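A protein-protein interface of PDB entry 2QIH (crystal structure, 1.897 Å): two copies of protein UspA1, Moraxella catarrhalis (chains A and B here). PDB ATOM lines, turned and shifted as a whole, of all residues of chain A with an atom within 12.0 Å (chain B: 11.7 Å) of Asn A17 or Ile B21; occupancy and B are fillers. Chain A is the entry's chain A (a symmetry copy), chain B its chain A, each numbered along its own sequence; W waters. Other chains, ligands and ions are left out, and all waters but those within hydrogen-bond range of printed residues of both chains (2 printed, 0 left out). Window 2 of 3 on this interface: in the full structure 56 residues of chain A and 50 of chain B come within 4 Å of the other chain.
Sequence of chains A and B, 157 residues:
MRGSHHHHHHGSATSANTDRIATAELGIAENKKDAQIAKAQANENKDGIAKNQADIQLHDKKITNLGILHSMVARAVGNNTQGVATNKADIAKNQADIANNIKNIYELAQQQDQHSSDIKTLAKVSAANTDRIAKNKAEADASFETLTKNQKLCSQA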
ATOM      1  N   ASN A  17      24.502 -14.343  33.267  1.00  0.00           N
ATOM      2  CA  ASN A  17      23.625 -14.761  34.405  1.00  0.00           C
ATOM      3  C   ASN A  17      23.948 -16.181  34.864  1.00  0.00           C
ATOM      4  O   ASN A  17      23.740 -17.162  34.141  1.00  0.00           O
ATOM      5  CB  ASN A  17      22.144 -14.590  34.053  1.00  0.00           C
ATOM      6  CG  ASN A  17      21.199 -15.036  35.173  1.00  0.00           C
ATOM      7  OD1 ASN A  17      21.017 -16.224  35.391  1.00  0.00           O
ATOM      8  ND2 ASN A  17      20.546 -14.075  35.839  1.00  0.00           N
ATOM      9  N   THR A  18      24.437 -16.254  36.093  1.00  0.00           N
ATOM     10  CA  THR A  18      24.995 -17.469  36.661  1.00  0.00           C
ATOM     11  C   THR A  18      23.979 -18.599  36.794  1.00  0.00           C
ATOM     12  O   THR A  18      24.287 -19.758  36.491  1.00  0.00           O
ATOM     13  CB  THR A  18      25.662 -17.145  38.018  1.00  0.00           C
ATOM     14  OG1 THR A  18      26.788 -16.283  37.784  1.00  0.00           O
ATOM     15  CG2 THR A  18      26.128 -18.416  38.724  1.00  0.00           C
ATOM     16  N   ASP A  19      22.769 -18.255  37.237  1.00  0.00           N
ATOM     17  CA  ASP A  19      21.710 -19.237  37.428  1.00  0.00           C
ATOM     18  C   ASP A  19      21.321 -19.900  36.088  1.00  0.00           C
ATOM     19  O   ASP A  19      20.951 -21.078  36.053  1.00  0.00           O
ATOM     20  CB  ASP A  19      20.478 -18.595  38.072  1.00  0.00           C
ATOM     21  CG  ASP A  19      20.758 -17.991  39.454  1.00  0.00           C
ATOM     22  OD1 ASP A  19      21.941 -17.858  39.844  1.00  0.00           O
ATOM     23  OD2 ASP A  19      19.771 -17.632  40.144  1.00  0.00           O
ATOM     24  N   ARG A  20      21.393 -19.135  35.002  1.00  0.00           N
ATOM     25  CA  ARG A  20      21.035 -19.659  33.678  1.00  0.00           C
ATOM     26  C   ARG A  20      22.122 -20.624  33.170  1.00  0.00           C
ATOM     27  O   ARG A  20      21.828 -21.704  32.637  1.00  0.00           O
ATOM     28  CB  ARG A  20      20.803 -18.505  32.694  1.00  0.00           C
ATOM     29  CG  ARG A  20      19.523 -17.716  32.989  1.00  0.00           C
ATOM     30  CD  ARG A  20      19.372 -16.506  32.103  1.00  0.00           C
ATOM     31  NE  ARG A  20      18.913 -16.864  30.758  1.00  0.00           N
ATOM     32  CZ  ARG A  20      18.862 -16.016  29.738  1.00  0.00           C
ATOM     33  NH1 ARG A  20      19.244 -14.752  29.902  1.00  0.00           N
ATOM     34  NH2 ARG A  20      18.437 -16.428  28.560  1.00  0.00           N
ATOM     35  N   ILE A  21      23.368 -20.207  33.325  1.00  0.00           N
ATOM     36  CA  ILE A  21      24.535 -21.053  33.018  1.00  0.00           C
ATOM     37  C   ILE A  21      24.472 -22.366  33.778  1.00  0.00           C
ATOM     38  O   ILE A  21      24.682 -23.429  33.197  1.00  0.00           O
ATOM     39  CB  ILE A  21      25.869 -20.297  33.282  1.00  0.00           C
ATOM     40  CG1 ILE A  21      25.932 -19.069  32.371  1.00  0.00           C
ATOM     41  CG2 ILE A  21      27.100 -21.214  33.068  1.00  0.00           C
ATOM     42  CD1 ILE A  21      27.231 -18.228  32.449  1.00  0.00           C
ATOM     43  N   ALA A  22      24.155 -22.298  35.073  1.00  0.00           N
ATOM     44  CA  ALA A  22      24.120 -23.501  35.918  1.00  0.00           C
ATOM     45  C   ALA A  22      23.116 -24.522  35.386  1.00  0.00           C
ATOM     46  O   ALA A  22      23.393 -25.696  35.293  1.00  0.00           O
ATOM     47  CB  ALA A  22      23.774 -23.141  37.363  1.00  0.00           C
ATOM     48  N   THR A  23      21.931 -24.046  35.068  1.00  0.00           N
ATOM     49  CA  THR A  23      20.849 -24.894  34.567  1.00  0.00           C
ATOM     50  C   THR A  23      21.238 -25.516  33.232  1.00  0.00           C
ATOM     51  O   THR A  23      20.945 -26.685  32.955  1.00  0.00           O
ATOM     52  CB  THR A  23      19.592 -24.036  34.406  1.00  0.00           C
ATOM     53  OG1 THR A  23      19.243 -23.483  35.686  1.00  0.00           O
ATOM     54  CG2 THR A  23      18.422 -24.855  33.859  1.00  0.00           C
ATOM     55  N   ALA A  24      21.907 -24.710  32.420  1.00  0.00           N
ATOM     56  CA  ALA A  24      22.324 -25.107  31.097  1.00  0.00           C
ATOM     57  C   ALA A  24      23.356 -26.250  31.156  1.00  0.00           C
ATOM     58  O   ALA A  24      23.228 -27.223  30.406  1.00  0.00           O
ATOM     59  CB  ALA A  24      22.859 -23.901  30.334  1.00  0.00           C
ATOM     60  N   GLU A  25      24.310 -26.157  32.096  1.00  0.00           N
ATOM     61  CA  GLU A  25      25.341 -27.199  32.289  1.00  0.00           C
ATOM     62  C   GLU A  25      24.769 -28.584  32.599  1.00  0.00           C
ATOM     63  O   GLU A  25      25.202 -29.614  32.026  1.00  0.00           O
ATOM     64  CB  GLU A  25      26.353 -26.791  33.378  1.00  0.00           C
ATOM     65  CG  GLU A  25      27.127 -25.494  33.055  1.00  0.00           C
ATOM     66  CD  GLU A  25      28.014 -25.014  34.215  1.00  0.00           C
ATOM     67  OE1 GLU A  25      27.697 -25.313  35.387  1.00  0.00           O
ATOM     68  OE2 GLU A  25      29.042 -24.362  33.950  1.00  0.00           O
ATOM     69  N   LEU A  26      23.774 -28.611  33.494  1.00  0.00           N
ATOM     70  CA  LEU A  26      23.045 -29.815  33.814  1.00  0.00           C
ATOM     71  C   LEU A  26      22.317 -30.352  32.586  1.00  0.00           C
ATOM     72  O   LEU A  26      22.330 -31.561  32.340  1.00  0.00           O
ATOM     73  CB  LEU A  26      22.032 -29.531  34.921  1.00  0.00           C
ATOM     74  CG  LEU A  26      22.495 -29.588  36.401  1.00  0.00           C
ATOM     75  CD1 LEU A  26      23.984 -29.495  36.578  1.00  0.00           C
ATOM     76  CD2 LEU A  26      21.755 -28.584  37.262  1.00  0.00           C
ATOM     77  N   GLY A  27      21.698 -29.455  31.807  1.00  0.00           N
ATOM     78  CA  GLY A  27      20.963 -29.904  30.629  1.00  0.00           C
ATOM     79  C   GLY A  27      21.887 -30.581  29.621  1.00  0.00           C
ATOM     80  O   GLY A  27      21.533 -31.574  29.021  1.00  0.00           O
ATOM     81  N   ILE A  28      23.066 -30.009  29.439  1.00  0.00           N
ATOM     82  CA  ILE A  28      24.048 -30.491  28.470  1.00  0.00           C
ATOM     83  C   ILE A  28      24.575 -31.850  28.904  1.00  0.00           C
ATOM     84  O   ILE A  28      24.697 -32.773  28.086  1.00  0.00           O
ATOM     85  CB  ILE A  28      25.202 -29.421  28.306  1.00  0.00           C
ATOM     86  CG1 ILE A  28      24.646 -28.147  27.670  1.00  0.00           C
ATOM     87  CG2 ILE A  28      26.385 -29.974  27.552  1.00  0.00           C
ATOM     88  CD1 ILE A  28      25.624 -26.926  27.836  1.00  0.00           C
ATOM     89  N   ASN B  17      27.663 -13.312  29.333  1.00  0.00           N
ATOM     90  CA  ASN B  17      27.051 -12.683  28.122  1.00  0.00           C
ATOM     91  C   ASN B  17      25.684 -13.285  27.810  1.00  0.00           C
ATOM     92  O   ASN B  17      25.557 -14.462  27.453  1.00  0.00           O
ATOM     93  CB  ASN B  17      28.001 -12.755  26.921  1.00  0.00           C
ATOM     94  CG  ASN B  17      27.410 -12.154  25.643  1.00  0.00           C
ATOM     95  OD1 ASN B  17      26.557 -12.759  25.013  1.00  0.00           O
ATOM     96  ND2 ASN B  17      27.918 -10.986  25.226  1.00  0.00           N
ATOM     97  N   THR B  18      24.676 -12.434  27.937  1.00  0.00           N
ATOM     98  CA  THR B  18      23.281 -12.834  27.886  1.00  0.00           C
ATOM     99  C   THR B  18      22.866 -13.419  26.539  1.00  0.00           C
ATOM    100  O   THR B  18      22.147 -14.424  26.487  1.00  0.00           O
ATOM    101  CB  THR B  18      22.387 -11.635  28.279  1.00  0.00           C
ATOM    102  OG1 THR B  18      22.637 -11.306  29.656  1.00  0.00           O
ATOM    103  CG2 THR B  18      20.908 -11.962  28.093  1.00  0.00           C
ATOM    104  N   ASP B  19      23.331 -12.795  25.456  1.00  0.00           N
ATOM    105  CA  ASP B  19      22.998 -13.238  24.109  1.00  0.00           C
ATOM    106  C   ASP B  19      23.539 -14.661  23.844  1.00  0.00           C
ATOM    107  O   ASP B  19      22.926 -15.439  23.107  1.00  0.00           O
ATOM    108  CB  ASP B  19      23.548 -12.266  23.061  1.00  0.00           C
ATOM    109  CG  ASP B  19      22.988 -10.844  23.197  1.00  0.00           C
ATOM    110  OD1 ASP B  19      22.343 -10.527  24.222  1.00  0.00           O
ATOM    111  OD2 ASP B  19      23.218 -10.036  22.262  1.00  0.00           O
ATOM    112  N   ARG B  20      24.687 -14.981  24.434  1.00  0.00           N
ATOM    113  CA  ARG B  20      25.297 -16.302  24.243  1.00  0.00           C
ATOM    114  C   ARG B  20      24.509 -17.376  25.013  1.00  0.00           C
ATOM    115  O   ARG B  20      24.235 -18.470  24.498  1.00  0.00           O
ATOM    116  CB  ARG B  20      26.771 -16.274  24.667  1.00  0.00           C
ATOM    117  CG  ARG B  20      27.655 -15.465  23.710  1.00  0.00           C
ATOM    118  CD  ARG B  20      29.072 -15.331  24.205  1.00  0.00           C
ATOM    119  NE  ARG B  20      29.849 -16.554  23.984  1.00  0.00           N
ATOM    120  CZ  ARG B  20      31.065 -16.763  24.476  1.00  0.00           C
ATOM    121  NH1 ARG B  20      31.651 -15.831  25.223  1.00  0.00           N
ATOM    122  NH2 ARG B  20      31.689 -17.897  24.227  1.00  0.00           N
ATOM    123  N   ILE B  21      24.173 -17.054  26.251  1.00  0.00           N
ATOM    124  CA  ILE B  21      23.306 -17.902  27.089  1.00  0.00           C
ATOM    125  C   ILE B  21      21.986 -18.187  26.394  1.00  0.00           C
ATOM    126  O   ILE B  21      21.543 -19.333  26.352  1.00  0.00           O
ATOM    127  CB  ILE B  21      23.094 -17.280  28.498  1.00  0.00           C
ATOM    128  CG1 ILE B  21      24.448 -17.164  29.199  1.00  0.00           C
ATOM    129  CG2 ILE B  21      22.095 -18.108  29.347  1.00  0.00           C
ATOM    130  CD1 ILE B  21      24.422 -16.623  30.651  1.00  0.00           C
ATOM    131  N   ALA B  22      21.371 -17.150  25.822  1.00  0.00           N
ATOM    132  CA  ALA B  22      20.060 -17.301  25.172  1.00  0.00           C
ATOM    133  C   ALA B  22      20.122 -18.318  24.032  1.00  0.00           C
ATOM    134  O   ALA B  22      19.276 -19.173  23.897  1.00  0.00           O
ATOM    135  CB  ALA B  22      19.560 -15.958  24.639  1.00  0.00           C
ATOM    136  N   THR B  23      21.132 -18.181  23.199  1.00  0.00           N
ATOM    137  CA  THR B  23      21.323 -19.055  22.041  1.00  0.00           C
ATOM    138  C   THR B  23      21.562 -20.490  22.496  1.00  0.00           C
ATOM    139  O   THR B  23      21.071 -21.449  21.888  1.00  0.00           O
ATOM    140  CB  THR B  23      22.521 -18.546  21.239  1.00  0.00           C
ATOM    141  OG1 THR B  23      22.253 -17.202  20.809  1.00  0.00           O
ATOM    142  CG2 THR B  23      22.797 -19.433  20.022  1.00  0.00           C
ATOM    143  N   ALA B  24      22.321 -20.608  23.576  1.00  0.00           N
ATOM    144  CA  ALA B  24      22.693 -21.889  24.131  1.00  0.00           C
ATOM    145  C   ALA B  24      21.458 -22.649  24.656  1.00  0.00           C
ATOM    146  O   ALA B  24      21.321 -23.844  24.379  1.00  0.00           O
ATOM    147  CB  ALA B  24      23.745 -21.701  25.217  1.00  0.00           C
ATOM    148  N   GLU B  25      20.546 -21.932  25.329  1.00  0.00           N
ATOM    149  CA  GLU B  25      19.298 -22.525  25.855  1.00  0.00           C
ATOM    150  C   GLU B  25      18.420 -23.169  24.782  1.00  0.00           C
ATOM    151  O   GLU B  25      17.899 -24.299  24.953  1.00  0.00           O
ATOM    152  CB  GLU B  25      18.480 -21.491  26.657  1.00  0.00           C
ATOM    153  CG  GLU B  25      19.225 -20.926  27.886  1.00  0.00           C
ATOM    154  CD  GLU B  25      18.464 -19.786  28.582  1.00  0.00           C
ATOM    155  OE1 GLU B  25      17.677 -19.082  27.911  1.00  0.00           O
ATOM    156  OE2 GLU B  25      18.634 -19.613  29.804  1.00  0.00           O
ATOM    157  N   LEU B  26      18.268 -22.459  23.658  1.00  0.00           N
ATOM    158  CA  LEU B  26      17.570 -22.969  22.502  1.00  0.00           C
ATOM    159  C   LEU B  26      18.267 -24.206  21.946  1.00  0.00           C
ATOM    160  O   LEU B  26      17.603 -25.185  21.596  1.00  0.00           O
ATOM    161  CB  LEU B  26      17.504 -21.894  21.418  1.00  0.00           C
ATOM    162  CG  LEU B  26      16.364 -20.842  21.466  1.00  0.00           C
ATOM    163  CD1 LEU B  26      15.695 -20.728  22.806  1.00  0.00           C
ATOM    164  CD2 LEU B  26      16.819 -19.495  20.938  1.00  0.00           C
ATOM    165  N   GLY B  27      19.605 -24.171  21.881  1.00  0.00           N
ATOM    166  CA  GLY B  27      20.333 -25.313  21.340  1.00  0.00           C
ATOM    167  C   GLY B  27      20.112 -26.566  22.183  1.00  0.00           C
ATOM    168  O   GLY B  27      19.962 -27.650  21.659  1.00  0.00           O
ATOM    169  N   ILE B  28      20.115 -26.391  23.494  1.00  0.00           N
ATOM    170  CA  ILE B  28      19.976 -27.489  24.447  1.00  0.00           C
ATOM    171  C   ILE B  28      18.579 -28.083  24.350  1.00  0.00           C
ATOM    172  O   ILE B  28      18.411 -29.310  24.333  1.00  0.00           O
ATOM    173  CB  ILE B  28      20.311 -26.973  25.905  1.00  0.00           C
ATOM    174  CG1 ILE B  28      21.788 -26.587  25.995  1.00  0.00           C
ATOM    175  CG2 ILE B  28      19.909 -27.968  26.965  1.00  0.00           C
ATOM    176  CD1 ILE B  28      22.094 -25.714  27.267  1.00  0.00           C
ATOM    177  N   ALA B  29      17.563 -27.225  24.219  1.00  0.00           N
ATOM    178  CA  ALA B  29      16.238 -27.743  24.089  1.00  0.00           C
ATOM    179  C   ALA B  29      16.110 -28.523  22.775  1.00  0.00           C
ATOM    180  O   ALA B  29      15.487 -29.556  22.763  1.00  0.00           O
ATOM    181  CB  ALA B  29      15.175 -26.631  24.189  1.00  0.00           C
ATOM    182  N   GLU B  30      16.751 -28.056  21.693  1.00  0.00           N
ATOM    183  CA  GLU B  30      16.767 -28.790  20.425  1.00  0.00           C
ATOM    184  C   GLU B  30      17.436 -30.153  20.586  1.00  0.00           C
ATOM    185  O   GLU B  30      16.931 -31.180  20.128  1.00  0.00           O
ATOM    186  CB  GLU B  30      17.470 -27.939  19.338  1.00  0.00           C
ATOM    187  CG  GLU B  30      16.542 -26.761  18.868  1.00  0.00           C
ATOM    188  CD  GLU B  30      17.234 -25.674  18.044  1.00  0.00           C
ATOM    189  OE1 GLU B  30      18.493 -25.624  18.001  1.00  0.00           O
ATOM    190  OE2 GLU B  30      16.498 -24.850  17.435  1.00  0.00           O
HETATM  191  O   HOH W   1      19.160 -22.185  31.185  1.00  0.00           O
HETATM  192  O   HOH W   2      23.042 -13.328  31.614  1.00  0.00           O
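Among the printed residues, merely in contact across the chains: Asn A17 with Ile B21 (3.5 Å), Arg A20 with Thr B18 (3.7 Å), Arg A20 with Ile B21 (3.6 Å), Arg A20 with Ala B22 (3.9 Å), Ile A21 with Ile B21 (3.3 Å), Ala A24 with Ile B28 (3.6 Å) and Ile A28 with Ile B28 (3.5 Å).
Arg A20 touches Thr B18, but with the chains exchanged Thr A18 does not touch Arg B20 (11.1 Å). Arg A20 touches Ala B22, but with the chains exchanged Ala A22 does not touch Arg B20 (11.2 Å). Ala A24 touches Ile B28, but with the chains exchanged Ile A28 does not touch Ala B24 (6.1 Å). Ile B28 touches its own counterpart, Ile A28. Of the 8 pairs that touch across the chains among the printed residues, 2 have their exchanged pair printed and touching as well.
The side-chain carboxylate of Glu B25 lies within salt-bridge range of the guanidinium group of Arg A20 (2.8 Å).
OD1 of Asn A17 lies within hydrogen-bond range of N of Asp A19 (3.3 Å). The backbone NH (N) of Arg A20 lies within hydrogen-bond range of the side-chain amide oxygen (OD1) of Asn A17 (3.0 Å).
Asn A17 touches just one residue of chain B: Ile B21 (3.5 Å). Ile B21 touches just these residues of chain A: Asn A17 (3.5 Å), Arg A20 (3.6 Å) and Ile A21 (3.3 Å). No residue of chain B comes within 4 Å of Thr A18. Arg A20 touches just these residues of chain B: Thr B18, Ile B21, Ala B22 and Glu B25. Ile A21 touches just one residue of chain B: Ile B21 (3.3 Å). Asn B17 touches none of the printed residues of chain A. No residue of chain A comes within 4 Å of Arg B20. No residue of chain A comes within 4 Å of Ala B24. Glu B25 touches one residue of chain A. Of the printed residues of chain B, Ile A28 touches Ile B28. Of the printed residues of chain A, Ile B28 touches Ala A24 and Ile A28.
Water W2 lies within hydrogen-bond range of N of Asn A17 (2.4 Å) and OG1 of Thr B18 (2.8 Å). Water W1 lies within hydrogen-bond range of the side-chain carboxylate of Glu B25 (3.0 Å) and the backbone carbonyl oxygen of Arg A20 (3.1 Å).
Of the 14 printed residues of chain B, 5 touch a printed residue of chain A. Along chain B the printed residues that touch a printed residue of chain A span positions 18 to 28. Among the printed residues, 8 pairs touch across the chains.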
